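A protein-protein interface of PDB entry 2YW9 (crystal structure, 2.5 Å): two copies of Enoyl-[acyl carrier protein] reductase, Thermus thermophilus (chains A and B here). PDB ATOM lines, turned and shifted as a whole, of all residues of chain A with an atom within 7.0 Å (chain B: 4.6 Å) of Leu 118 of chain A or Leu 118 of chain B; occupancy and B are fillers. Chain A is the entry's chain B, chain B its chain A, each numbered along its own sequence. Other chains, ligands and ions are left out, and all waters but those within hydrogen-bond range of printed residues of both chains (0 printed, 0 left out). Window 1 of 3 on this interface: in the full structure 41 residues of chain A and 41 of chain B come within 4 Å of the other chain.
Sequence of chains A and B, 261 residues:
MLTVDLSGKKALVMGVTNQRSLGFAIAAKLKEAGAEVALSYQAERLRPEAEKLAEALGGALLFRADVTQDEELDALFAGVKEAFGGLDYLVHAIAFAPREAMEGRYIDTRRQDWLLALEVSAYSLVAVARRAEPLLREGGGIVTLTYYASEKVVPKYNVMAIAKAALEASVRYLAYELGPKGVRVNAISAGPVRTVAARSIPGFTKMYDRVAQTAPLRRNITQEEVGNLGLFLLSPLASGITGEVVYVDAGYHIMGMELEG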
ATOM      1  N   PHE A  96     -22.127 -11.373 -13.013  1.00  0.00           N
ATOM      2  CA  PHE A  96     -22.234 -12.605 -13.771  1.00  0.00           C
ATOM      3  C   PHE A  96     -22.827 -13.729 -12.942  1.00  0.00           C
ATOM      4  O   PHE A  96     -22.488 -13.902 -11.770  1.00  0.00           O
ATOM      5  CB  PHE A  96     -20.863 -13.039 -14.296  1.00  0.00           C
ATOM      6  CG  PHE A  96     -20.872 -14.384 -14.971  1.00  0.00           C
ATOM      7  CD1 PHE A  96     -21.371 -14.524 -16.260  1.00  0.00           C
ATOM      8  CD2 PHE A  96     -20.388 -15.510 -14.317  1.00  0.00           C
ATOM      9  CE1 PHE A  96     -21.393 -15.764 -16.883  1.00  0.00           C
ATOM     10  CE2 PHE A  96     -20.406 -16.752 -14.935  1.00  0.00           C
ATOM     11  CZ  PHE A  96     -20.909 -16.878 -16.218  1.00  0.00           C
ATOM     12  N   ALA A  97     -23.714 -14.491 -13.567  1.00  0.00           N
ATOM     13  CA  ALA A  97     -24.193 -15.740 -13.016  1.00  0.00           C
ATOM     14  C   ALA A  97     -24.332 -16.676 -14.204  1.00  0.00           C
ATOM     15  O   ALA A  97     -24.800 -16.254 -15.256  1.00  0.00           O
ATOM     16  CB  ALA A  97     -25.522 -15.540 -12.329  1.00  0.00           C
ATOM     17  N   PRO A  98     -23.913 -17.941 -14.051  1.00  0.00           N
ATOM     18  CA  PRO A  98     -24.007 -18.912 -15.137  1.00  0.00           C
ATOM     19  C   PRO A  98     -25.432 -19.052 -15.657  1.00  0.00           C
ATOM     20  O   PRO A  98     -26.388 -18.867 -14.899  1.00  0.00           O
ATOM     21  CB  PRO A  98     -23.558 -20.216 -14.480  1.00  0.00           C
ATOM     22  CG  PRO A  98     -22.706 -19.795 -13.346  1.00  0.00           C
ATOM     23  CD  PRO A  98     -23.321 -18.528 -12.839  1.00  0.00           C
ATOM     24  N   TYR A 106     -34.500 -20.691  -8.137  1.00  0.00           N
ATOM     25  CA  TYR A 106     -33.351 -20.423  -7.288  1.00  0.00           C
ATOM     26  C   TYR A 106     -32.974 -21.653  -6.470  1.00  0.00           C
ATOM     27  O   TYR A 106     -31.790 -21.934  -6.250  1.00  0.00           O
ATOM     28  CB  TYR A 106     -33.635 -19.234  -6.354  1.00  0.00           C
ATOM     29  CG  TYR A 106     -32.548 -18.997  -5.332  1.00  0.00           C
ATOM     30  CD1 TYR A 106     -32.808 -19.087  -3.968  1.00  0.00           C
ATOM     31  CD2 TYR A 106     -31.250 -18.711  -5.734  1.00  0.00           C
ATOM     32  CE1 TYR A 106     -31.802 -18.883  -3.037  1.00  0.00           C
ATOM     33  CE2 TYR A 106     -30.241 -18.507  -4.815  1.00  0.00           C
ATOM     34  CZ  TYR A 106     -30.519 -18.592  -3.467  1.00  0.00           C
ATOM     35  OH  TYR A 106     -29.502 -18.382  -2.557  1.00  0.00           O
ATOM     36  N   GLN A 112     -21.725 -25.179  -7.700  1.00  0.00           N
ATOM     37  CA  GLN A 112     -20.616 -24.442  -8.292  1.00  0.00           C
ATOM     38  C   GLN A 112     -21.073 -23.241  -9.107  1.00  0.00           C
ATOM     39  O   GLN A 112     -20.338 -22.253  -9.227  1.00  0.00           O
ATOM     40  CB  GLN A 112     -19.718 -25.366  -9.112  1.00  0.00           C
ATOM     41  CG  GLN A 112     -19.141 -26.553  -8.320  1.00  0.00           C
ATOM     42  CD  GLN A 112     -18.172 -26.144  -7.205  1.00  0.00           C
ATOM     43  OE1 GLN A 112     -17.379 -25.210  -7.354  1.00  0.00           O
ATOM     44  NE2 GLN A 112     -18.228 -26.862  -6.089  1.00  0.00           N
ATOM     45  N   ASP A 113     -22.282 -23.321  -9.660  1.00  0.00           N
ATOM     46  CA  ASP A 113     -22.891 -22.170 -10.323  1.00  0.00           C
ATOM     47  C   ASP A 113     -23.158 -21.066  -9.310  1.00  0.00           C
ATOM     48  O   ASP A 113     -22.845 -19.900  -9.550  1.00  0.00           O
ATOM     49  CB  ASP A 113     -24.206 -22.558 -10.998  1.00  0.00           C
ATOM     50  CG  ASP A 113     -23.996 -23.364 -12.259  1.00  0.00           C
ATOM     51  OD1 ASP A 113     -22.844 -23.418 -12.738  1.00  0.00           O
ATOM     52  OD2 ASP A 113     -24.987 -23.930 -12.779  1.00  0.00           O
ATOM     53  N   TRP A 114     -23.745 -21.448  -8.180  1.00  0.00           N
ATOM     54  CA  TRP A 114     -24.040 -20.513  -7.096  1.00  0.00           C
ATOM     55  C   TRP A 114     -22.768 -19.817  -6.619  1.00  0.00           C
ATOM     56  O   TRP A 114     -22.727 -18.591  -6.511  1.00  0.00           O
ATOM     57  CB  TRP A 114     -24.715 -21.258  -5.939  1.00  0.00           C
ATOM     58  CG  TRP A 114     -25.353 -20.399  -4.897  1.00  0.00           C
ATOM     59  CD1 TRP A 114     -26.671 -20.037  -4.825  1.00  0.00           C
ATOM     60  CD2 TRP A 114     -24.716 -19.827  -3.743  1.00  0.00           C
ATOM     61  NE1 TRP A 114     -26.889 -19.264  -3.708  1.00  0.00           N
ATOM     62  CE2 TRP A 114     -25.706 -19.120  -3.027  1.00  0.00           C
ATOM     63  CE3 TRP A 114     -23.403 -19.840  -3.251  1.00  0.00           C
ATOM     64  CZ2 TRP A 114     -25.425 -18.428  -1.846  1.00  0.00           C
ATOM     65  CZ3 TRP A 114     -23.124 -19.150  -2.074  1.00  0.00           C
ATOM     66  CH2 TRP A 114     -24.131 -18.453  -1.387  1.00  0.00           C
ATOM     67  N   LEU A 115     -21.727 -20.597  -6.352  1.00  0.00           N
ATOM     68  CA  LEU A 115     -20.480 -20.045  -5.829  1.00  0.00           C
ATOM     69  C   LEU A 115     -19.811 -19.114  -6.834  1.00  0.00           C
ATOM     70  O   LEU A 115     -19.242 -18.084  -6.455  1.00  0.00           O
ATOM     71  CB  LEU A 115     -19.519 -21.164  -5.410  1.00  0.00           C
ATOM     72  CG  LEU A 115     -19.932 -21.932  -4.152  1.00  0.00           C
ATOM     73  CD1 LEU A 115     -19.233 -23.286  -4.089  1.00  0.00           C
ATOM     74  CD2 LEU A 115     -19.663 -21.108  -2.881  1.00  0.00           C
ATOM     75  N   LEU A 116     -19.885 -19.477  -8.113  1.00  0.00           N
ATOM     76  CA  LEU A 116     -19.261 -18.682  -9.164  1.00  0.00           C
ATOM     77  C   LEU A 116     -19.964 -17.335  -9.310  1.00  0.00           C
ATOM     78  O   LEU A 116     -19.311 -16.299  -9.448  1.00  0.00           O
ATOM     79  CB  LEU A 116     -19.278 -19.429 -10.498  1.00  0.00           C
ATOM     80  CG  LEU A 116     -18.495 -18.777 -11.642  1.00  0.00           C
ATOM     81  CD1 LEU A 116     -17.025 -18.611 -11.269  1.00  0.00           C
ATOM     82  CD2 LEU A 116     -18.647 -19.581 -12.923  1.00  0.00           C
ATOM     83  N   ALA A 117     -21.294 -17.363  -9.277  1.00  0.00           N
ATOM     84  CA  ALA A 117     -22.093 -16.152  -9.340  1.00  0.00           C
ATOM     85  C   ALA A 117     -21.692 -15.212  -8.215  1.00  0.00           C
ATOM     86  O   ALA A 117     -21.481 -14.017  -8.428  1.00  0.00           O
ATOM     87  CB  ALA A 117     -23.569 -16.483  -9.252  1.00  0.00           C
ATOM     88  N   LEU A 118     -21.572 -15.760  -7.014  1.00  0.00           N
ATOM     89  CA  LEU A 118     -21.173 -14.953  -5.874  1.00  0.00           C
ATOM     90  C   LEU A 118     -19.724 -14.495  -5.948  1.00  0.00           C
ATOM     91  O   LEU A 118     -19.388 -13.401  -5.502  1.00  0.00           O
ATOM     92  CB  LEU A 118     -21.501 -15.653  -4.557  1.00  0.00           C
ATOM     93  CG  LEU A 118     -22.903 -15.203  -4.138  1.00  0.00           C
ATOM     94  CD1 LEU A 118     -23.963 -16.201  -4.561  1.00  0.00           C
ATOM     95  CD2 LEU A 118     -22.974 -14.944  -2.653  1.00  0.00           C
ATOM     96  N   GLU A 119     -18.873 -15.322  -6.535  1.00  0.00           N
ATOM     97  CA  GLU A 119     -17.453 -14.988  -6.668  1.00  0.00           C
ATOM     98  C   GLU A 119     -17.233 -13.798  -7.597  1.00  0.00           C
ATOM     99  O   GLU A 119     -16.516 -12.858  -7.258  1.00  0.00           O
ATOM    100  CB  GLU A 119     -16.662 -16.195  -7.179  1.00  0.00           C
ATOM    101  CG  GLU A 119     -15.159 -16.044  -7.033  1.00  0.00           C
ATOM    102  CD  GLU A 119     -14.388 -17.207  -7.624  1.00  0.00           C
ATOM    103  OE1 GLU A 119     -13.161 -17.262  -7.425  1.00  0.00           O
ATOM    104  OE2 GLU A 119     -15.001 -18.064  -8.289  1.00  0.00           O
ATOM    105  N   VAL A 120     -17.852 -13.855  -8.769  1.00  0.00           N
ATOM    106  CA  VAL A 120     -17.714 -12.808  -9.771  1.00  0.00           C
ATOM    107  C   VAL A 120     -18.503 -11.543  -9.397  1.00  0.00           C
ATOM    108  O   VAL A 120     -18.026 -10.426  -9.587  1.00  0.00           O
ATOM    109  CB  VAL A 120     -18.154 -13.319 -11.175  1.00  0.00           C
ATOM    110  CG1 VAL A 120     -18.051 -12.219 -12.213  1.00  0.00           C
ATOM    111  CG2 VAL A 120     -17.308 -14.505 -11.600  1.00  0.00           C
ATOM    112  N   SER A 121     -19.699 -11.730  -8.845  1.00  0.00           N
ATOM    113  CA  SER A 121     -20.606 -10.612  -8.607  1.00  0.00           C
ATOM    114  C   SER A 121     -20.429  -9.922  -7.257  1.00  0.00           C
ATOM    115  O   SER A 121     -20.660  -8.718  -7.145  1.00  0.00           O
ATOM    116  CB  SER A 121     -22.063 -11.049  -8.786  1.00  0.00           C
ATOM    117  OG  SER A 121     -22.296 -11.574 -10.084  1.00  0.00           O
ATOM    118  N   ALA A 122     -20.036 -10.665  -6.229  1.00  0.00           N
ATOM    119  CA  ALA A 122     -19.872 -10.052  -4.907  1.00  0.00           C
ATOM    120  C   ALA A 122     -18.420  -9.988  -4.426  1.00  0.00           C
ATOM    121  O   ALA A 122     -17.936  -8.911  -4.094  1.00  0.00           O
ATOM    122  CB  ALA A 122     -20.775 -10.724  -3.865  1.00  0.00           C
ATOM    123  N   TYR A 123     -17.727 -11.131  -4.411  1.00  0.00           N
ATOM    124  CA  TYR A 123     -16.353 -11.179  -3.890  1.00  0.00           C
ATOM    125  C   TYR A 123     -15.387 -10.287  -4.658  1.00  0.00           C
ATOM    126  O   TYR A 123     -14.437  -9.752  -4.085  1.00  0.00           O
ATOM    127  CB  TYR A 123     -15.791 -12.612  -3.827  1.00  0.00           C
ATOM    128  CG  TYR A 123     -14.385 -12.605  -3.281  1.00  0.00           C
ATOM    129  CD1 TYR A 123     -14.148 -12.322  -1.933  1.00  0.00           C
ATOM    130  CD2 TYR A 123     -13.293 -12.805  -4.111  1.00  0.00           C
ATOM    131  CE1 TYR A 123     -12.865 -12.275  -1.422  1.00  0.00           C
ATOM    132  CE2 TYR A 123     -12.002 -12.745  -3.612  1.00  0.00           C
ATOM    133  CZ  TYR A 123     -11.795 -12.483  -2.263  1.00  0.00           C
ATOM    134  OH  TYR A 123     -10.516 -12.431  -1.763  1.00  0.00           O
ATOM    135  N   SER A 124     -15.627 -10.133  -5.956  1.00  0.00           N
ATOM    136  CA  SER A 124     -14.765  -9.308  -6.790  1.00  0.00           C
ATOM    137  C   SER A 124     -14.660  -7.889  -6.258  1.00  0.00           C
ATOM    138  O   SER A 124     -13.659  -7.228  -6.481  1.00  0.00           O
ATOM    139  CB  SER A 124     -15.269  -9.275  -8.232  1.00  0.00           C
ATOM    140  OG  SER A 124     -16.477  -8.541  -8.325  1.00  0.00           O
ATOM    141  N   VAL A 159     -30.109 -16.312  -8.279  1.00  0.00           N
ATOM    142  CA  VAL A 159     -28.875 -16.126  -7.516  1.00  0.00           C
ATOM    143  C   VAL A 159     -28.279 -14.718  -7.643  1.00  0.00           C
ATOM    144  O   VAL A 159     -27.505 -14.278  -6.784  1.00  0.00           O
ATOM    145  CB  VAL A 159     -27.819 -17.195  -7.890  1.00  0.00           C
ATOM    146  CG1 VAL A 159     -27.372 -17.026  -9.339  1.00  0.00           C
ATOM    147  CG2 VAL A 159     -26.623 -17.140  -6.946  1.00  0.00           C
ATOM    148  N   MET A 160     -28.638 -14.000  -8.700  1.00  0.00           N
ATOM    149  CA  MET A 160     -28.142 -12.639  -8.841  1.00  0.00           C
ATOM    150  C   MET A 160     -28.655 -11.752  -7.704  1.00  0.00           C
ATOM    151  O   MET A 160     -27.949 -10.859  -7.241  1.00  0.00           O
ATOM    152  CB  MET A 160     -28.498 -12.049 -10.208  1.00  0.00           C
ATOM    153  CG  MET A 160     -27.503 -12.374 -11.320  1.00  0.00           C
ATOM    154  SD  MET A 160     -25.755 -12.117 -10.911  1.00  0.00           S
ATOM    155  CE  MET A 160     -25.686 -10.361 -10.570  1.00  0.00           C
ATOM    156  N   ILE A 162     -29.284 -12.718  -4.662  1.00  0.00           N
ATOM    157  CA  ILE A 162     -28.516 -13.116  -3.502  1.00  0.00           C
ATOM    158  C   ILE A 162     -27.151 -12.470  -3.576  1.00  0.00           C
ATOM    159  O   ILE A 162     -26.665 -11.913  -2.597  1.00  0.00           O
ATOM    160  CB  ILE A 162     -28.356 -14.646  -3.480  1.00  0.00           C
ATOM    161  CG1 ILE A 162     -29.695 -15.309  -3.809  1.00  0.00           C
ATOM    162  CG2 ILE A 162     -27.785 -15.131  -2.152  1.00  0.00           C
ATOM    163  CD1 ILE A 162     -30.798 -15.015  -2.837  1.00  0.00           C
ATOM    164  N   ALA A 163     -26.543 -12.523  -4.754  1.00  0.00           N
ATOM    165  CA  ALA A 163     -25.241 -11.905  -4.974  1.00  0.00           C
ATOM    166  C   ALA A 163     -25.298 -10.402  -4.717  1.00  0.00           C
ATOM    167  O   ALA A 163     -24.370  -9.826  -4.141  1.00  0.00           O
ATOM    168  CB  ALA A 163     -24.747 -12.185  -6.386  1.00  0.00           C
ATOM    169  N   LYS A 164     -26.391  -9.772  -5.137  1.00  0.00           N
ATOM    170  CA  LYS A 164     -26.558  -8.340  -4.926  1.00  0.00           C
ATOM    171  C   LYS A 164     -26.739  -8.013  -3.454  1.00  0.00           C
ATOM    172  O   LYS A 164     -26.304  -6.960  -2.996  1.00  0.00           O
ATOM    173  CB  LYS A 164     -27.739  -7.794  -5.733  1.00  0.00           C
ATOM    174  CG  LYS A 164     -27.480  -7.728  -7.233  1.00  0.00           C
ATOM    175  CD  LYS A 164     -26.097  -7.171  -7.573  1.00  0.00           C
ATOM    176  CE  LYS A 164     -25.954  -6.943  -9.071  1.00  0.00           C
ATOM    177  NZ  LYS A 164     -24.631  -6.358  -9.447  1.00  0.00           N
ATOM    178  N   ALA A 166     -25.392  -9.837  -1.034  1.00  0.00           N
ATOM    179  CA  ALA A 166     -24.028 -10.001  -0.537  1.00  0.00           C
ATOM    180  C   ALA A 166     -23.168  -8.801  -0.913  1.00  0.00           C
ATOM    181  O   ALA A 166     -22.280  -8.405  -0.161  1.00  0.00           O
ATOM    182  CB  ALA A 166     -23.413 -11.279  -1.076  1.00  0.00           C
ATOM    183  N   LEU A 167     -23.450  -8.223  -2.078  1.00  0.00           N
ATOM    184  CA  LEU A 167     -22.702  -7.069  -2.568  1.00  0.00           C
ATOM    185  C   LEU A 167     -22.971  -5.822  -1.738  1.00  0.00           C
ATOM    186  O   LEU A 167     -22.045  -5.086  -1.426  1.00  0.00           O
ATOM    187  CB  LEU A 167     -23.035  -6.793  -4.036  1.00  0.00           C
ATOM    188  CG  LEU A 167     -22.281  -5.660  -4.735  1.00  0.00           C
ATOM    189  CD1 LEU A 167     -20.779  -5.937  -4.761  1.00  0.00           C
ATOM    190  CD2 LEU A 167     -22.812  -5.439  -6.148  1.00  0.00           C
ATOM    191  N   TRP B 114     -13.635 -16.854   1.799  1.00  0.00           N
ATOM    192  CA  TRP B 114     -14.874 -16.148   1.529  1.00  0.00           C
ATOM    193  C   TRP B 114     -15.887 -17.087   0.889  1.00  0.00           C
ATOM    194  O   TRP B 114     -17.042 -17.135   1.312  1.00  0.00           O
ATOM    195  CB  TRP B 114     -14.594 -14.966   0.602  1.00  0.00           C
ATOM    196  CG  TRP B 114     -15.696 -13.955   0.470  1.00  0.00           C
ATOM    197  CD1 TRP B 114     -15.829 -12.790   1.171  1.00  0.00           C
ATOM    198  CD2 TRP B 114     -16.802 -13.998  -0.450  1.00  0.00           C
ATOM    199  NE1 TRP B 114     -16.950 -12.113   0.754  1.00  0.00           N
ATOM    200  CE2 TRP B 114     -17.563 -12.828  -0.243  1.00  0.00           C
ATOM    201  CE3 TRP B 114     -17.218 -14.910  -1.424  1.00  0.00           C
ATOM    202  CZ2 TRP B 114     -18.717 -12.545  -0.975  1.00  0.00           C
ATOM    203  CZ3 TRP B 114     -18.374 -14.626  -2.157  1.00  0.00           C
ATOM    204  CH2 TRP B 114     -19.107 -13.455  -1.923  1.00  0.00           C
ATOM    205  N   LEU B 115     -15.457 -17.848  -0.113  1.00  0.00           N
ATOM    206  CA  LEU B 115     -16.380 -18.738  -0.814  1.00  0.00           C
ATOM    207  C   LEU B 115     -16.866 -19.850   0.105  1.00  0.00           C
ATOM    208  O   LEU B 115     -18.048 -20.211   0.100  1.00  0.00           O
ATOM    209  CB  LEU B 115     -15.735 -19.314  -2.076  1.00  0.00           C
ATOM    210  CG  LEU B 115     -15.538 -18.326  -3.229  1.00  0.00           C
ATOM    211  CD1 LEU B 115     -14.469 -18.829  -4.185  1.00  0.00           C
ATOM    212  CD2 LEU B 115     -16.861 -18.067  -3.959  1.00  0.00           C
ATOM    213  N   LEU B 116     -15.955 -20.371   0.917  1.00  0.00           N
ATOM    214  CA  LEU B 116     -16.296 -21.465   1.808  1.00  0.00           C
ATOM    215  C   LEU B 116     -17.329 -21.023   2.834  1.00  0.00           C
ATOM    216  O   LEU B 116     -18.278 -21.754   3.120  1.00  0.00           O
ATOM    217  CB  LEU B 116     -15.051 -22.002   2.512  1.00  0.00           C
ATOM    218  CG  LEU B 116     -15.271 -23.291   3.315  1.00  0.00           C
ATOM    219  CD1 LEU B 116     -15.949 -24.386   2.470  1.00  0.00           C
ATOM    220  CD2 LEU B 116     -13.944 -23.784   3.897  1.00  0.00           C
ATOM    221  N   ALA B 117     -17.134 -19.823   3.378  1.00  0.00           N
ATOM    222  CA  ALA B 117     -18.046 -19.266   4.369  1.00  0.00           C
ATOM    223  C   ALA B 117     -19.453 -19.138   3.798  1.00  0.00           C
ATOM    224  O   ALA B 117     -20.435 -19.478   4.455  1.00  0.00           O
ATOM    225  CB  ALA B 117     -17.544 -17.919   4.853  1.00  0.00           C
ATOM    226  N   LEU B 118     -19.542 -18.658   2.565  1.00  0.00           N
ATOM    227  CA  LEU B 118     -20.830 -18.507   1.916  1.00  0.00           C
ATOM    228  C   LEU B 118     -21.436 -19.828   1.483  1.00  0.00           C
ATOM    229  O   LEU B 118     -22.660 -19.956   1.424  1.00  0.00           O
ATOM    230  CB  LEU B 118     -20.741 -17.537   0.736  1.00  0.00           C
ATOM    231  CG  LEU B 118     -21.054 -16.125   1.220  1.00  0.00           C
ATOM    232  CD1 LEU B 118     -19.790 -15.359   1.575  1.00  0.00           C
ATOM    233  CD2 LEU B 118     -21.837 -15.396   0.187  1.00  0.00           C
ATOM    234  N   GLU B 119     -20.575 -20.808   1.197  1.00  0.00           N
ATOM    235  CA  GLU B 119     -21.024 -22.138   0.816  1.00  0.00           C
ATOM    236  C   GLU B 119     -21.720 -22.839   1.972  1.00  0.00           C
ATOM    237  O   GLU B 119     -22.862 -23.319   1.833  1.00  0.00           O
ATOM    238  CB  GLU B 119     -19.856 -22.991   0.338  1.00  0.00           C
ATOM    239  CG  GLU B 119     -20.306 -24.250  -0.370  1.00  0.00           C
ATOM    240  CD  GLU B 119     -19.160 -25.165  -0.726  1.00  0.00           C
ATOM    241  OE1 GLU B 119     -19.427 -26.220  -1.349  1.00  0.00           O
ATOM    242  OE2 GLU B 119     -18.004 -24.839  -0.382  1.00  0.00           O
ATOM    243  N   VAL B 120     -21.028 -22.886   3.110  1.00  0.00           N
ATOM    244  CA  VAL B 120     -21.522 -23.563   4.303  1.00  0.00           C
ATOM    245  C   VAL B 120     -22.660 -22.780   4.954  1.00  0.00           C
ATOM    246  O   VAL B 120     -23.641 -23.363   5.416  1.00  0.00           O
ATOM    247  CB  VAL B 120     -20.384 -23.777   5.342  1.00  0.00           C
ATOM    248  CG1 VAL B 120     -20.912 -24.448   6.587  1.00  0.00           C
ATOM    249  CG2 VAL B 120     -19.249 -24.601   4.754  1.00  0.00           C
ATOM    250  N   SER B 121     -22.543 -21.455   4.968  1.00  0.00           N
ATOM    251  CA  SER B 121     -23.491 -20.630   5.717  1.00  0.00           C
ATOM    252  C   SER B 121     -24.721 -20.175   4.937  1.00  0.00           C
ATOM    253  O   SER B 121     -25.765 -19.916   5.534  1.00  0.00           O
ATOM    254  CB  SER B 121     -22.788 -19.414   6.329  1.00  0.00           C
ATOM    255  OG  SER B 121     -21.669 -19.801   7.108  1.00  0.00           O
ATOM    256  N   ALA B 122     -24.611 -20.060   3.616  1.00  0.00           N
ATOM    257  CA  ALA B 122     -25.755 -19.590   2.822  1.00  0.00           C
ATOM    258  C   ALA B 122     -26.258 -20.615   1.812  1.00  0.00           C
ATOM    259  O   ALA B 122     -27.441 -20.931   1.796  1.00  0.00           O
ATOM    260  CB  ALA B 122     -25.446 -18.257   2.138  1.00  0.00           C
ATOM    261  N   TYR B 123     -25.368 -21.145   0.979  1.00  0.00           N
ATOM    262  CA  TYR B 123     -25.800 -22.097  -0.041  1.00  0.00           C
ATOM    263  C   TYR B 123     -26.400 -23.377   0.534  1.00  0.00           C
ATOM    264  O   TYR B 123     -27.261 -24.000  -0.087  1.00  0.00           O
ATOM    265  CB  TYR B 123     -24.678 -22.464  -1.021  1.00  0.00           C
ATOM    266  CG  TYR B 123     -25.180 -23.452  -2.054  1.00  0.00           C
ATOM    267  CD1 TYR B 123     -26.101 -23.056  -3.021  1.00  0.00           C
ATOM    268  CD2 TYR B 123     -24.788 -24.788  -2.029  1.00  0.00           C
ATOM    269  CE1 TYR B 123     -26.590 -23.946  -3.956  1.00  0.00           C
ATOM    270  CE2 TYR B 123     -25.279 -25.690  -2.958  1.00  0.00           C
ATOM    271  CZ  TYR B 123     -26.179 -25.259  -3.918  1.00  0.00           C
ATOM    272  OH  TYR B 123     -26.672 -26.137  -4.850  1.00  0.00           O
ATOM    273  N   VAL B 159     -17.080 -11.694   7.108  1.00  0.00           N
ATOM    274  CA  VAL B 159     -17.775 -12.417   6.041  1.00  0.00           C
ATOM    275  C   VAL B 159     -19.057 -13.102   6.500  1.00  0.00           C
ATOM    276  O   VAL B 159     -19.912 -13.435   5.673  1.00  0.00           O
ATOM    277  CB  VAL B 159     -16.838 -13.459   5.371  1.00  0.00           C
ATOM    278  CG1 VAL B 159     -16.472 -14.564   6.351  1.00  0.00           C
ATOM    279  CG2 VAL B 159     -17.481 -14.042   4.125  1.00  0.00           C
ATOM    280  N   ALA B 163     -22.566 -13.479   4.610  1.00  0.00           N
ATOM    281  CA  ALA B 163     -23.216 -14.777   4.477  1.00  0.00           C
ATOM    282  C   ALA B 163     -24.663 -14.700   4.953  1.00  0.00           C
ATOM    283  O   ALA B 163     -25.566 -15.248   4.322  1.00  0.00           O
ATOM    284  CB  ALA B 163     -22.454 -15.848   5.259  1.00  0.00           C
ATOM    285  N   ALA B 166     -26.786 -12.922   2.473  1.00  0.00           N
ATOM    286  CA  ALA B 166     -27.067 -13.891   1.419  1.00  0.00           C
ATOM    287  C   ALA B 166     -28.107 -14.911   1.875  1.00  0.00           C
ATOM    288  O   ALA B 166     -28.929 -15.375   1.087  1.00  0.00           O
ATOM    289  CB  ALA B 166     -25.775 -14.596   0.996  1.00  0.00           C
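N of Tyr 123 of chain B is in hydrogen-bond range of O of Leu 118 of chain B (3.0 Å).
OH of Tyr 106 of chain A sits at hydrogen-bond distance from NE1 of Trp 114 of chain A.
N of Tyr 123 of chain A is in hydrogen-bond range of O of Leu 118 of chain A, 3.0 Å away.
The backbone carbonyl oxygen of Glu 119 of chain A sits at hydrogen-bond distance from the backbone NH of Ser 124 of chain A (3.1 Å).
Leu 118 of chain A touches two residues of chain B.
Of the printed residues of chain B, Trp 114 of chain A touches Leu 118, Ala 122 and Tyr 123.
Of the printed residues of chain A, Ala 122 of chain B touches Trp 114.
Val 159 of chain B touches none of the printed residues of chain A.
Leu 116 of chain B touches none of the printed residues of chain A.
The nearest printed residue of chain B that does not touch Leu 118 of chain A is Ala 166 of chain B (4.6 Å).
The nearest residue of chain A that does not touch Leu 118 of chain B is Ala 166 of chain A (4.6 Å).
Trp 114 of chain A touches Leu 118 of chain B (CH2 to O, 3.5 Å).
Trp 114 of chain A touches Ala 122 of chain B.
CD1 of Tyr 123 of chain B touches CG of Trp 114 of chain A, 3.3 Å away.
Leu 115 of chain B touches Leu 115 of chain A.
Leu 118 of chain A touches Trp 114 of chain B.
Leu 118 of chain A touches Leu 118 of chain B (CD2 to CD2, 3.1 Å).
Leu 115 of chain B touches Glu 119 of chain A (CD2 to CB, 3.7 Å).
CB of Ala 122 of chain A touches CH2 of Trp 114 of chain B, at 3.7 Å.
Trp 114 of chain B touches Tyr 123 of chain A.
O of Ala 166 of chain B touches CG2 of Ile 162 of chain A (3.4 Å).
Of the 24 printed residues of chain A, 7 touch a printed residue of chain B.
Printed residues of chain B that touch a printed residue of chain A: Trp 114, Leu 115, Leu 118, Glu 119, Ala 122, Tyr 123 and Ala 166.
Hydrophobic or aromatic side chains of chain B that line the printed part of chain A: Trp 114, Leu 115, Leu 118, Ala 122, Tyr 123 and Ala 166.
Along chain B the printed residues that touch a printed residue of chain A span positions 114 to 166.
Among the printed residues, no Asp or Glu carboxylate lies within 4 Å of a Lys or Arg side-chain nitrogen of the other chain.
Trp 114 of chain A touches Leu 118 of chain B, and with the chains exchanged Leu 118 of chain A touches Trp 114 of chain B.
Trp 114 of chain A touches Tyr 123 of chain B, and with the chains exchanged Tyr 123 of chain A touches Trp 114 of chain B.
Leu 115 of chain A touches its own counterpart, Leu 115 of chain B.
Leu 115 of chain A touches Glu 119 of chain B, and with the chains exchanged Glu 119 of chain A touches Leu 115 of chain B.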
